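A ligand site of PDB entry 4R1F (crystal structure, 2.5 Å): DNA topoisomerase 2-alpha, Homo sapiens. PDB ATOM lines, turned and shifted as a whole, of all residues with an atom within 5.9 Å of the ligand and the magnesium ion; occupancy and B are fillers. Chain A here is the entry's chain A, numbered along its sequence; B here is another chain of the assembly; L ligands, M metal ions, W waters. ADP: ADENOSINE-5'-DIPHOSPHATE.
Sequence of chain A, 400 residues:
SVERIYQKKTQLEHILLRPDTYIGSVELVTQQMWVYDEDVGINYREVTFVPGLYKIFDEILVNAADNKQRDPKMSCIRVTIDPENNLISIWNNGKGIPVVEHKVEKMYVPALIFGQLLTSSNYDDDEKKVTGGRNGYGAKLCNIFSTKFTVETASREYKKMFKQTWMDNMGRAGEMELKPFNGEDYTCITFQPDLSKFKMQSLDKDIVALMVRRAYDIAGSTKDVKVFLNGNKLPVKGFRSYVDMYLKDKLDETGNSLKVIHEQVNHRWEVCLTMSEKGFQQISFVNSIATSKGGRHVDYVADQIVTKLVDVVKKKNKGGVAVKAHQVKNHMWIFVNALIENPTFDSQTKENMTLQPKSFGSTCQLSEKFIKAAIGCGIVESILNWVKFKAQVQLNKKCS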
ATOM      1  N   GLU A  59      14.513 -24.341  37.183  1.00  0.00           N
ATOM      2  CA  GLU A  59      14.606 -23.552  35.977  1.00  0.00           C
ATOM      3  C   GLU A  59      13.742 -24.117  34.841  1.00  0.00           C
ATOM      4  O   GLU A  59      13.068 -23.370  34.105  1.00  0.00           O
ATOM      5  CB  GLU A  59      16.072 -23.419  35.534  1.00  0.00           C
ATOM      6  CG  GLU A  59      16.968 -22.513  36.425  1.00  0.00           C
ATOM      7  CD  GLU A  59      16.382 -21.113  36.684  1.00  0.00           C
ATOM      8  OE1 GLU A  59      15.688 -20.525  35.790  1.00  0.00           O
ATOM      9  OE2 GLU A  59      16.578 -20.583  37.792  1.00  0.00           O
ATOM     10  N   ILE A  60      13.748 -25.432  34.707  1.00  0.00           N
ATOM     11  CA  ILE A  60      12.983 -26.066  33.662  1.00  0.00           C
ATOM     12  C   ILE A  60      11.480 -26.091  34.003  1.00  0.00           C
ATOM     13  O   ILE A  60      10.613 -25.877  33.151  1.00  0.00           O
ATOM     14  CB  ILE A  60      13.472 -27.469  33.408  1.00  0.00           C
ATOM     15  CG1 ILE A  60      14.996 -27.501  33.124  1.00  0.00           C
ATOM     16  CG2 ILE A  60      12.699 -28.082  32.263  1.00  0.00           C
ATOM     17  CD1 ILE A  60      15.451 -26.564  32.041  1.00  0.00           C
ATOM     18  N   VAL A  62       9.852 -23.805  35.988  1.00  0.00           N
ATOM     19  CA  VAL A  62       9.348 -22.460  35.806  1.00  0.00           C
ATOM     20  C   VAL A  62       9.171 -22.103  34.318  1.00  0.00           C
ATOM     21  O   VAL A  62       8.250 -21.408  33.931  1.00  0.00           O
ATOM     22  CB  VAL A  62      10.218 -21.434  36.533  1.00  0.00           C
ATOM     23  CG1 VAL A  62       9.796 -20.008  36.193  1.00  0.00           C
ATOM     24  CG2 VAL A  62      10.089 -21.640  38.035  1.00  0.00           C
ATOM     25  N   ASN A  63      10.082 -22.587  33.479  1.00  0.00           N
ATOM     26  CA  ASN A  63       9.984 -22.331  32.051  1.00  0.00           C
ATOM     27  C   ASN A  63       8.700 -22.863  31.505  1.00  0.00           C
ATOM     28  O   ASN A  63       8.072 -22.219  30.663  1.00  0.00           O
ATOM     29  CB  ASN A  63      11.161 -22.968  31.313  1.00  0.00           C
ATOM     30  CG  ASN A  63      12.390 -22.067  31.300  1.00  0.00           C
ATOM     31  OD1 ASN A  63      12.297 -20.869  31.586  1.00  0.00           O
ATOM     32  ND2 ASN A  63      13.536 -22.643  31.006  1.00  0.00           N
ATOM     33  N   ALA A  64       8.280 -24.027  31.982  1.00  0.00           N
ATOM     34  CA  ALA A  64       7.007 -24.613  31.553  1.00  0.00           C
ATOM     35  C   ALA A  64       5.853 -23.745  31.976  1.00  0.00           C
ATOM     36  O   ALA A  64       5.001 -23.409  31.172  1.00  0.00           O
ATOM     37  CB  ALA A  64       6.859 -25.990  32.111  1.00  0.00           C
ATOM     38  N   ASP A  66       6.076 -20.531  32.523  1.00  0.00           N
ATOM     39  CA  ASP A  66       6.168 -19.286  31.780  1.00  0.00           C
ATOM     40  C   ASP A  66       5.361 -19.415  30.464  1.00  0.00           C
ATOM     41  O   ASP A  66       4.754 -18.443  30.006  1.00  0.00           O
ATOM     42  CB  ASP A  66       7.629 -18.924  31.479  1.00  0.00           C
ATOM     43  CG  ASP A  66       8.361 -18.465  32.689  1.00  0.00           C
ATOM     44  OD1 ASP A  66       7.703 -18.027  33.672  1.00  0.00           O
ATOM     45  OD2 ASP A  66       9.643 -18.470  32.658  1.00  0.00           O
ATOM     46  N   ASN A  67       5.360 -20.606  29.866  1.00  0.00           N
ATOM     47  CA  ASN A  67       4.662 -20.781  28.609  1.00  0.00           C
ATOM     48  C   ASN A  67       3.159 -20.484  28.666  1.00  0.00           C
ATOM     49  O   ASN A  67       2.533 -20.262  27.640  1.00  0.00           O
ATOM     50  CB  ASN A  67       4.871 -22.161  28.049  1.00  0.00           C
ATOM     51  CG  ASN A  67       4.730 -22.195  26.540  1.00  0.00           C
ATOM     52  OD1 ASN A  67       5.390 -21.431  25.848  1.00  0.00           O
ATOM     53  ND2 ASN A  67       3.863 -23.081  26.033  1.00  0.00           N
ATOM     54  N   ARG A  70       2.795 -16.870  27.611  1.00  0.00           N
ATOM     55  CA  ARG A  70       2.992 -16.870  26.183  1.00  0.00           C
ATOM     56  C   ARG A  70       1.754 -17.378  25.425  1.00  0.00           C
ATOM     57  O   ARG A  70       1.441 -16.892  24.330  1.00  0.00           O
ATOM     58  CB  ARG A  70       4.194 -17.741  25.847  1.00  0.00           C
ATOM     59  CG  ARG A  70       4.486 -17.845  24.369  1.00  0.00           C
ATOM     60  CD  ARG A  70       5.879 -18.358  24.083  1.00  0.00           C
ATOM     61  NE  ARG A  70       5.988 -18.861  22.711  1.00  0.00           N
ATOM     62  CZ  ARG A  70       5.899 -20.140  22.365  1.00  0.00           C
ATOM     63  NH1 ARG A  70       5.678 -21.090  23.276  1.00  0.00           N
ATOM     64  NH2 ARG A  70       6.054 -20.488  21.086  1.00  0.00           N
ATOM     65  N   ASN A  92       5.132 -29.897  28.685  1.00  0.00           N
ATOM     66  CA  ASN A  92       4.013 -28.959  28.729  1.00  0.00           C
ATOM     67  C   ASN A  92       3.337 -28.899  27.367  1.00  0.00           C
ATOM     68  O   ASN A  92       3.950 -29.185  26.336  1.00  0.00           O
ATOM     69  CB  ASN A  92       4.434 -27.543  29.169  1.00  0.00           C
ATOM     70  CG  ASN A  92       5.390 -26.883  28.190  1.00  0.00           C
ATOM     71  OD1 ASN A  92       6.608 -27.105  28.228  1.00  0.00           O
ATOM     72  ND2 ASN A  92       4.845 -26.088  27.284  1.00  0.00           N
ATOM     73  N   LYS A  95       1.516 -23.544  22.885  1.00  0.00           N
ATOM     74  CA  LYS A  95       2.394 -23.335  21.693  1.00  0.00           C
ATOM     75  C   LYS A  95       3.800 -23.843  21.926  1.00  0.00           C
ATOM     76  O   LYS A  95       4.380 -23.640  23.008  1.00  0.00           O
ATOM     77  CB  LYS A  95       2.475 -21.864  21.269  1.00  0.00           C
ATOM     78  CG  LYS A  95       1.567 -21.527  20.122  1.00  0.00           C
ATOM     79  CD  LYS A  95       1.820 -20.118  19.610  1.00  0.00           C
ATOM     80  CE  LYS A  95       0.784 -19.658  18.627  1.00  0.00           C
ATOM     81  NZ  LYS A  95       0.347 -20.721  17.673  1.00  0.00           N
ATOM     82  N   GLY A  96       4.316 -24.534  20.933  1.00  0.00           N
ATOM     83  CA  GLY A  96       5.684 -25.061  20.937  1.00  0.00           C
ATOM     84  C   GLY A  96       6.654 -23.971  20.493  1.00  0.00           C
ATOM     85  O   GLY A  96       6.253 -22.863  20.136  1.00  0.00           O
ATOM     86  N   ILE A  97       7.935 -24.282  20.522  1.00  0.00           N
ATOM     87  CA  ILE A  97       8.940 -23.310  20.159  1.00  0.00           C
ATOM     88  C   ILE A  97       9.036 -23.337  18.622  1.00  0.00           C
ATOM     89  O   ILE A  97       9.104 -24.414  18.036  1.00  0.00           O
ATOM     90  CB  ILE A  97      10.287 -23.629  20.829  1.00  0.00           C
ATOM     91  CG1 ILE A  97      10.146 -23.554  22.345  1.00  0.00           C
ATOM     92  CG2 ILE A  97      11.380 -22.661  20.366  1.00  0.00           C
ATOM     93  CD1 ILE A  97      11.105 -24.472  23.063  1.00  0.00           C
ATOM     94  N   ILE A 113      18.206 -21.402  21.894  1.00  0.00           N
ATOM     95  CA  ILE A 113      17.761 -20.983  23.235  1.00  0.00           C
ATOM     96  C   ILE A 113      17.956 -22.050  24.337  1.00  0.00           C
ATOM     97  O   ILE A 113      17.833 -21.766  25.530  1.00  0.00           O
ATOM     98  CB  ILE A 113      16.325 -20.461  23.234  1.00  0.00           C
ATOM     99  CG1 ILE A 113      15.323 -21.590  23.022  1.00  0.00           C
ATOM    100  CG2 ILE A 113      16.200 -19.345  22.197  1.00  0.00           C
ATOM    101  CD1 ILE A 113      13.955 -21.079  22.683  1.00  0.00           C
ATOM    102  N   PHE A 114      18.339 -23.255  23.936  1.00  0.00           N
ATOM    103  CA  PHE A 114      18.715 -24.286  24.894  1.00  0.00           C
ATOM    104  C   PHE A 114      20.208 -24.621  24.872  1.00  0.00           C
ATOM    105  O   PHE A 114      20.713 -25.237  25.811  1.00  0.00           O
ATOM    106  CB  PHE A 114      17.887 -25.550  24.691  1.00  0.00           C
ATOM    107  CG  PHE A 114      16.466 -25.417  25.156  1.00  0.00           C
ATOM    108  CD1 PHE A 114      16.129 -25.648  26.487  1.00  0.00           C
ATOM    109  CD2 PHE A 114      15.480 -25.065  24.280  1.00  0.00           C
ATOM    110  CE1 PHE A 114      14.822 -25.539  26.915  1.00  0.00           C
ATOM    111  CE2 PHE A 114      14.176 -24.958  24.698  1.00  0.00           C
ATOM    112  CZ  PHE A 114      13.845 -25.178  26.007  1.00  0.00           C
ATOM    113  N   THR A 119      20.553 -16.286  25.913  1.00  0.00           N
ATOM    114  CA  THR A 119      19.466 -16.332  24.935  1.00  0.00           C
ATOM    115  C   THR A 119      18.131 -16.385  25.612  1.00  0.00           C
ATOM    116  O   THR A 119      17.945 -17.171  26.528  1.00  0.00           O
ATOM    117  CB  THR A 119      19.580 -17.558  24.038  1.00  0.00           C
ATOM    118  OG1 THR A 119      19.815 -18.724  24.820  1.00  0.00           O
ATOM    119  CG2 THR A 119      20.748 -17.396  23.042  1.00  0.00           C
ATOM    120  N   SER A 120      17.208 -15.554  25.182  1.00  0.00           N
ATOM    121  CA  SER A 120      15.928 -15.392  25.872  1.00  0.00           C
ATOM    122  C   SER A 120      14.930 -14.688  25.009  1.00  0.00           C
ATOM    123  O   SER A 120      15.308 -13.927  24.121  1.00  0.00           O
ATOM    124  CB  SER A 120      16.111 -14.558  27.149  1.00  0.00           C
ATOM    125  OG  SER A 120      14.886 -14.350  27.826  1.00  0.00           O
ATOM    126  N   SER A 121      13.648 -14.951  25.251  1.00  0.00           N
ATOM    127  CA  SER A 121      12.564 -14.137  24.661  1.00  0.00           C
ATOM    128  C   SER A 121      12.057 -13.111  25.645  1.00  0.00           C
ATOM    129  O   SER A 121      11.105 -12.410  25.343  1.00  0.00           O
ATOM    130  CB  SER A 121      11.383 -14.997  24.197  1.00  0.00           C
ATOM    131  OG  SER A 121      10.879 -15.779  25.242  1.00  0.00           O
ATOM    132  N   ASN A 122      12.777 -12.939  26.751  1.00  0.00           N
ATOM    133  CA  ASN A 122      12.404 -11.950  27.759  1.00  0.00           C
ATOM    134  C   ASN A 122      13.422 -10.850  27.969  1.00  0.00           C
ATOM    135  O   ASN A 122      13.494 -10.263  29.043  1.00  0.00           O
ATOM    136  CB  ASN A 122      12.175 -12.645  29.079  1.00  0.00           C
ATOM    137  CG  ASN A 122      11.128 -13.732  28.995  1.00  0.00           C
ATOM    138  OD1 ASN A 122      10.021 -13.498  28.544  1.00  0.00           O
ATOM    139  ND2 ASN A 122      11.513 -14.967  29.357  1.00  0.00           N
ATOM    140  N   GLY A 132       8.670 -15.779  34.893  1.00  0.00           N
ATOM    141  CA  GLY A 132       9.804 -15.969  35.787  1.00  0.00           C
ATOM    142  C   GLY A 132      11.093 -15.732  35.035  1.00  0.00           C
ATOM    143  O   GLY A 132      12.110 -15.378  35.617  1.00  0.00           O
ATOM    144  N   GLY A 133      11.047 -15.989  33.736  1.00  0.00           N
ATOM    145  CA  GLY A 133      12.224 -15.826  32.890  1.00  0.00           C
ATOM    146  C   GLY A 133      12.585 -14.379  32.666  1.00  0.00           C
ATOM    147  O   GLY A 133      11.710 -13.528  32.477  1.00  0.00           O
ATOM    148  N   ARG A 134      13.880 -14.105  32.689  1.00  0.00           N
ATOM    149  CA  ARG A 134      14.372 -12.775  32.574  1.00  0.00           C
ATOM    150  C   ARG A 134      15.810 -12.721  32.073  1.00  0.00           C
ATOM    151  O   ARG A 134      16.146 -11.809  31.328  1.00  0.00           O
ATOM    152  CB  ARG A 134      14.220 -12.057  33.941  1.00  0.00           C
ATOM    153  CG  ARG A 134      14.361 -10.559  33.846  1.00  0.00           C
ATOM    154  CD  ARG A 134      13.862  -9.785  35.062  1.00  0.00           C
ATOM    155  NE  ARG A 134      14.653  -8.559  35.292  1.00  0.00           N
ATOM    156  CZ  ARG A 134      15.751  -8.467  36.056  1.00  0.00           C
ATOM    157  NH1 ARG A 134      16.253  -9.517  36.727  1.00  0.00           N
ATOM    158  NH2 ARG A 134      16.377  -7.298  36.142  1.00  0.00           N
ATOM    159  N   ASN A 135      16.660 -13.635  32.506  1.00  0.00           N
ATOM    160  CA  ASN A 135      18.108 -13.515  32.303  1.00  0.00           C
ATOM    161  C   ASN A 135      18.669 -14.350  31.177  1.00  0.00           C
ATOM    162  O   ASN A 135      19.756 -14.089  30.721  1.00  0.00           O
ATOM    163  CB  ASN A 135      18.888 -13.866  33.563  1.00  0.00           C
ATOM    164  CG  ASN A 135      18.534 -12.979  34.761  1.00  0.00           C
ATOM    165  OD1 ASN A 135      18.853 -11.806  34.790  1.00  0.00           O
ATOM    166  ND2 ASN A 135      17.901 -13.568  35.769  1.00  0.00           N
ATOM    167  N   GLY A 136      17.939 -15.318  30.681  1.00  0.00           N
ATOM    168  CA  GLY A 136      18.439 -16.152  29.590  1.00  0.00           C
ATOM    169  C   GLY A 136      19.531 -17.144  29.948  1.00  0.00           C
ATOM    170  O   GLY A 136      20.325 -17.548  29.083  1.00  0.00           O
ATOM    171  N   TYR A 137      19.595 -17.515  31.216  1.00  0.00           N
ATOM    172  CA  TYR A 137      20.563 -18.526  31.699  1.00  0.00           C
ATOM    173  C   TYR A 137      19.927 -19.912  31.929  1.00  0.00           C
ATOM    174  O   TYR A 137      20.508 -20.928  31.607  1.00  0.00           O
ATOM    175  CB  TYR A 137      21.248 -18.058  33.000  1.00  0.00           C
ATOM    176  CG  TYR A 137      22.571 -17.301  32.816  1.00  0.00           C
ATOM    177  CD1 TYR A 137      23.702 -17.954  32.341  1.00  0.00           C
ATOM    178  CD2 TYR A 137      22.691 -15.954  33.150  1.00  0.00           C
ATOM    179  CE1 TYR A 137      24.895 -17.282  32.175  1.00  0.00           C
ATOM    180  CE2 TYR A 137      23.881 -15.277  32.972  1.00  0.00           C
ATOM    181  CZ  TYR A 137      24.970 -15.957  32.489  1.00  0.00           C
ATOM    182  OH  TYR A 137      26.182 -15.302  32.311  1.00  0.00           O
ATOM    183  N   GLY A 138      18.764 -19.905  32.573  1.00  0.00           N
ATOM    184  CA  GLY A 138      18.185 -21.088  33.219  1.00  0.00           C
ATOM    185  C   GLY A 138      18.312 -22.422  32.512  1.00  0.00           C
ATOM    186  O   GLY A 138      18.884 -23.368  33.039  1.00  0.00           O
ATOM    187  N   ALA A 139      17.789 -22.495  31.310  1.00  0.00           N
ATOM    188  CA  ALA A 139      17.781 -23.735  30.580  1.00  0.00           C
ATOM    189  C   ALA A 139      19.181 -24.177  30.243  1.00  0.00           C
ATOM    190  O   ALA A 139      19.488 -25.388  30.263  1.00  0.00           O
ATOM    191  CB  ALA A 139      16.981 -23.577  29.315  1.00  0.00           C
ATOM    192  N   LYS A 140      20.057 -23.211  29.950  1.00  0.00           N
ATOM    193  CA  LYS A 140      21.453 -23.529  29.676  1.00  0.00           C
ATOM    194  C   LYS A 140      22.125 -24.099  30.929  1.00  0.00           C
ATOM    195  O   LYS A 140      22.902 -25.033  30.872  1.00  0.00           O
ATOM    196  CB  LYS A 140      22.211 -22.315  29.151  1.00  0.00           C
ATOM    197  CG  LYS A 140      22.050 -22.056  27.631  1.00  0.00           C
ATOM    198  CD  LYS A 140      20.640 -21.659  27.183  1.00  0.00           C
ATOM    199  CE  LYS A 140      20.292 -20.278  27.713  1.00  0.00           C
ATOM    200  NZ  LYS A 140      18.955 -19.858  27.293  1.00  0.00           N
ATOM    201  N   THR A 187       6.116 -29.293  24.375  1.00  0.00           N
ATOM    202  CA  THR A 187       7.557 -29.190  24.583  1.00  0.00           C
ATOM    203  C   THR A 187       7.891 -30.147  25.739  1.00  0.00           C
ATOM    204  O   THR A 187       7.239 -30.123  26.779  1.00  0.00           O
ATOM    205  CB  THR A 187       8.010 -27.750  24.913  1.00  0.00           C
ATOM    206  OG1 THR A 187       7.792 -26.857  23.791  1.00  0.00           O
ATOM    207  CG2 THR A 187       9.480 -27.718  25.225  1.00  0.00           C
ATOM    208  N   ILE A 189      11.341 -31.380  27.982  1.00  0.00           N
ATOM    209  CA  ILE A 189      12.769 -31.337  28.311  1.00  0.00           C
ATOM    210  C   ILE A 189      13.071 -32.516  29.220  1.00  0.00           C
ATOM    211  O   ILE A 189      12.434 -32.678  30.263  1.00  0.00           O
ATOM    212  CB  ILE A 189      13.167 -30.060  29.115  1.00  0.00           C
ATOM    213  CG1 ILE A 189      13.233 -28.802  28.258  1.00  0.00           C
ATOM    214  CG2 ILE A 189      14.585 -30.206  29.662  1.00  0.00           C
ATOM    215  CD1 ILE A 189      12.130 -28.587  27.253  1.00  0.00           C
ATOM    216  N   TYR B   6      13.246 -13.886  19.921  1.00  0.00           N
ATOM    217  CA  TYR B   6      14.325 -14.651  20.502  1.00  0.00           C
ATOM    218  C   TYR B   6      15.651 -14.000  20.231  1.00  0.00           C
ATOM    219  O   TYR B   6      16.101 -13.977  19.072  1.00  0.00           O
ATOM    220  CB  TYR B   6      14.340 -16.058  19.901  1.00  0.00           C
ATOM    221  CG  TYR B   6      13.068 -16.820  20.163  1.00  0.00           C
ATOM    222  CD1 TYR B   6      12.899 -17.526  21.324  1.00  0.00           C
ATOM    223  CD2 TYR B   6      12.023 -16.816  19.241  1.00  0.00           C
ATOM    224  CE1 TYR B   6      11.737 -18.228  21.587  1.00  0.00           C
ATOM    225  CE2 TYR B   6      10.870 -17.508  19.474  1.00  0.00           C
ATOM    226  CZ  TYR B   6      10.718 -18.220  20.651  1.00  0.00           C
ATOM    227  OH  TYR B   6       9.547 -18.939  20.893  1.00  0.00           O
HETATM  228  PB  ADP L   1      14.583 -17.137  30.452  1.00  0.00           P
HETATM  229  O1B ADP L   1      15.186 -16.183  31.388  1.00  0.00           O
HETATM  230  O2B ADP L   1      14.016 -16.476  29.214  1.00  0.00           O
HETATM  231  O3B ADP L   1      13.620 -18.119  30.997  1.00  0.00           O
HETATM  232  PA  ADP L   1      15.908 -19.614  29.884  1.00  0.00           P
HETATM  233  O1A ADP L   1      14.962 -20.363  30.701  1.00  0.00           O
HETATM  234  O2A ADP L   1      17.272 -20.146  29.751  1.00  0.00           O
HETATM  235  O3A ADP L   1      15.869 -18.023  30.132  1.00  0.00           O
HETATM  236  O5' ADP L   1      15.659 -19.649  28.344  1.00  0.00           O
HETATM  237  C5' ADP L   1      14.581 -20.338  27.850  1.00  0.00           C
HETATM  238  C4' ADP L   1      14.052 -19.579  26.660  1.00  0.00           C
HETATM  239  O4' ADP L   1      13.666 -20.621  25.812  1.00  0.00           O
HETATM  240  C3' ADP L   1      12.827 -18.763  27.051  1.00  0.00           C
HETATM  241  O3' ADP L   1      13.029 -17.356  26.945  1.00  0.00           O
HETATM  242  C2' ADP L   1      11.724 -19.218  26.154  1.00  0.00           C
HETATM  243  O2' ADP L   1      11.599 -18.346  25.019  1.00  0.00           O
HETATM  244  C1' ADP L   1      12.228 -20.598  25.721  1.00  0.00           C
HETATM  245  N9  ADP L   1      11.585 -21.714  26.463  1.00  0.00           N
HETATM  246  C8  ADP L   1      12.074 -22.397  27.483  1.00  0.00           C
HETATM  247  N7  ADP L   1      11.235 -23.356  27.880  1.00  0.00           N
HETATM  248  C5  ADP L   1      10.178 -23.273  27.100  1.00  0.00           C
HETATM  249  C6  ADP L   1       8.910 -24.004  26.990  1.00  0.00           C
HETATM  250  N6  ADP L   1       8.649 -25.005  27.834  1.00  0.00           N
HETATM  251  N1  ADP L   1       8.058 -23.634  26.033  1.00  0.00           N
HETATM  252  C2  ADP L   1       8.350 -22.621  25.185  1.00  0.00           C
HETATM  253  N3  ADP L   1       9.485 -21.931  25.221  1.00  0.00           N
HETATM  254  C4  ADP L   1      10.420 -22.209  26.145  1.00  0.00           C
HETATM  255 MG    MG M   1      13.874 -19.713  32.411  1.00  0.00          MG
HETATM  256  O   HOH W   1      10.517 -26.192  30.489  1.00  0.00           O
HETATM  257  O   HOH W   2      15.420 -18.435  33.186  1.00  0.00           O
HETATM  258  O   HOH W   3      12.212 -18.915  33.479  1.00  0.00           O
HETATM  259  O   HOH W   4      14.519 -21.087  33.923  1.00  0.00           O
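O1B of the ligand lies within hydrogen-bond range of N of Arg 134, 2.8 Å away.
The backbone NH (N) of Gly 138 sits at hydrogen-bond distance from an oxygen (O2A) of the ligand (3.2 Å).
The side-chain hydroxyl (OG) of Ser 121 is in hydrogen-bond range of an oxygen (O2') of the ligand, at 2.7 Å.
An oxygen (O1B) of the ligand sits at hydrogen-bond distance from the backbone NH of Asn 135 (3.1 Å).
O2B of the ligand is in hydrogen-bond range of OG of Ser 120.
An oxygen (O1B) of the ligand lies within hydrogen-bond range of the backbone NH of Gly 136.
OD1 of Asn 67 lies close to N1 of the ligand, at 3.5 Å.
The backbone NH of Ala 139 is in hydrogen-bond range of an oxygen (O2A) of the ligand, 2.9 Å away.
N of Ser 121 lies within hydrogen-bond range of O3' of the ligand (3.0 Å).
NZ of Lys 140 lies within salt-bridge range of O2A of the ligand.
N6 of the ligand lies within hydrogen-bond range of OD1 of Asn 92, 3.0 Å away.
O2B of the ligand lies within hydrogen-bond range of ND2 of Asn 122 (2.9 Å).
The backbone NH (N) of Asn 92 lies within hydrogen-bond range of the backbone carbonyl oxygen (O) of Thr 187 (2.9 Å).
The side-chain amino group (NZ) of Lys 140 is in hydrogen-bond range of the side-chain hydroxyl (OG1) of Thr 119, 2.9 Å away.
O of Gly 133 lies within hydrogen-bond range of ND2 of Asn 122 (3.4 Å).
O of Gly 96 lies within hydrogen-bond range of NH2 of Arg 70, 2.6 Å away.
O of Lys 95 is in hydrogen-bond range of ND2 of Asn 67 (3.1 Å).
O of Ile 113 is in hydrogen-bond range of NZ of Lys 140, at 2.8 Å.
The side-chain amide nitrogen (ND2) of Asn 67 sits close to the side-chain amide nitrogen (ND2) of Asn 92 (3.4 Å).
N of Thr 119 is in hydrogen-bond range of O of Gly 136, at 3.4 Å.
NH1 of Arg 70 touches C2 of the ligand (3.6 Å).
CG1 of Ile 97 touches N3 of the ligand (3.4 Å).
CD1 of Ile 113 touches O4' of the ligand, 3.2 Å away.
Phe 114 touches the ligand (CZ to C8, 3.6 Å).
O of Thr 119 touches O5' of the ligand, 3.8 Å away.
CA of Gly 133 touches O3B of the ligand, 3.3 Å away.
Tyr 137 touches the ligand.
Thr 187 touches the ligand.
CE1 of Tyr 6 of chain B touches O2' of the ligand, 3.4 Å away.
Hydrophobic or aromatic side chains that line the ligand: Ile 97, Ile 113, Phe 114, Ala 139 and Tyr 6 of chain B.
21 residues have an atom within 4 Å of the ligand: Asn 63, Asn 67, Arg 70, Asn 92, Ile 97, Ile 113, Phe 114, Thr 119, Ser 120, Ser 121, Asn 122, Gly 133, Arg 134, Asn 135, Gly 136, Tyr 137, Gly 138, Ala 139, Lys 140, Thr 187 and Tyr 6 of chain B.
OE1 of Glu 59 touches the magnesium ion, at 3.9 Å.
Within 4 Å of the magnesium ion: Glu 59 and Asn 63.
The nearest printed residue that does not touch the magnesium ion is Gly 133 (4.2 Å).
The side-chain amide oxygen (OD1) of Asn 63 binds the magnesium ion (2.1 Å).
The magnesium ion is bound by O1A of the ligand, 2.1 Å away.
Water W3 is bound to the magnesium ion (2.1 Å).
Water W4 is bound to the magnesium ion (2.1 Å).
O3B of the ligand is bound to the magnesium ion, 2.1 Å away.
Water W2 binds the magnesium ion (2.2 Å).
The magnesium ion has six donor atoms within binding distance.
Water W3 bridges the side-chain carboxylate of Asp 66 and the backbone NH of Gly 133.
Water W2 lies within hydrogen-bond range of O1B of the ligand (2.9 Å) and OE1 of Glu 59 (3.3 Å).
Water W4 lies within hydrogen-bond range of the backbone carbonyl oxygen (O) of Glu 59 (2.7 Å) and the side-chain amide nitrogen (ND2) of Asn 63 (3.4 Å).
Water W1 lies within hydrogen-bond range of the backbone carbonyl oxygen of Ile 60 (2.7 Å), the backbone NH of Ala 64 (3.5 Å) and a nitrogen (N6) of the ligand (3.5 Å).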
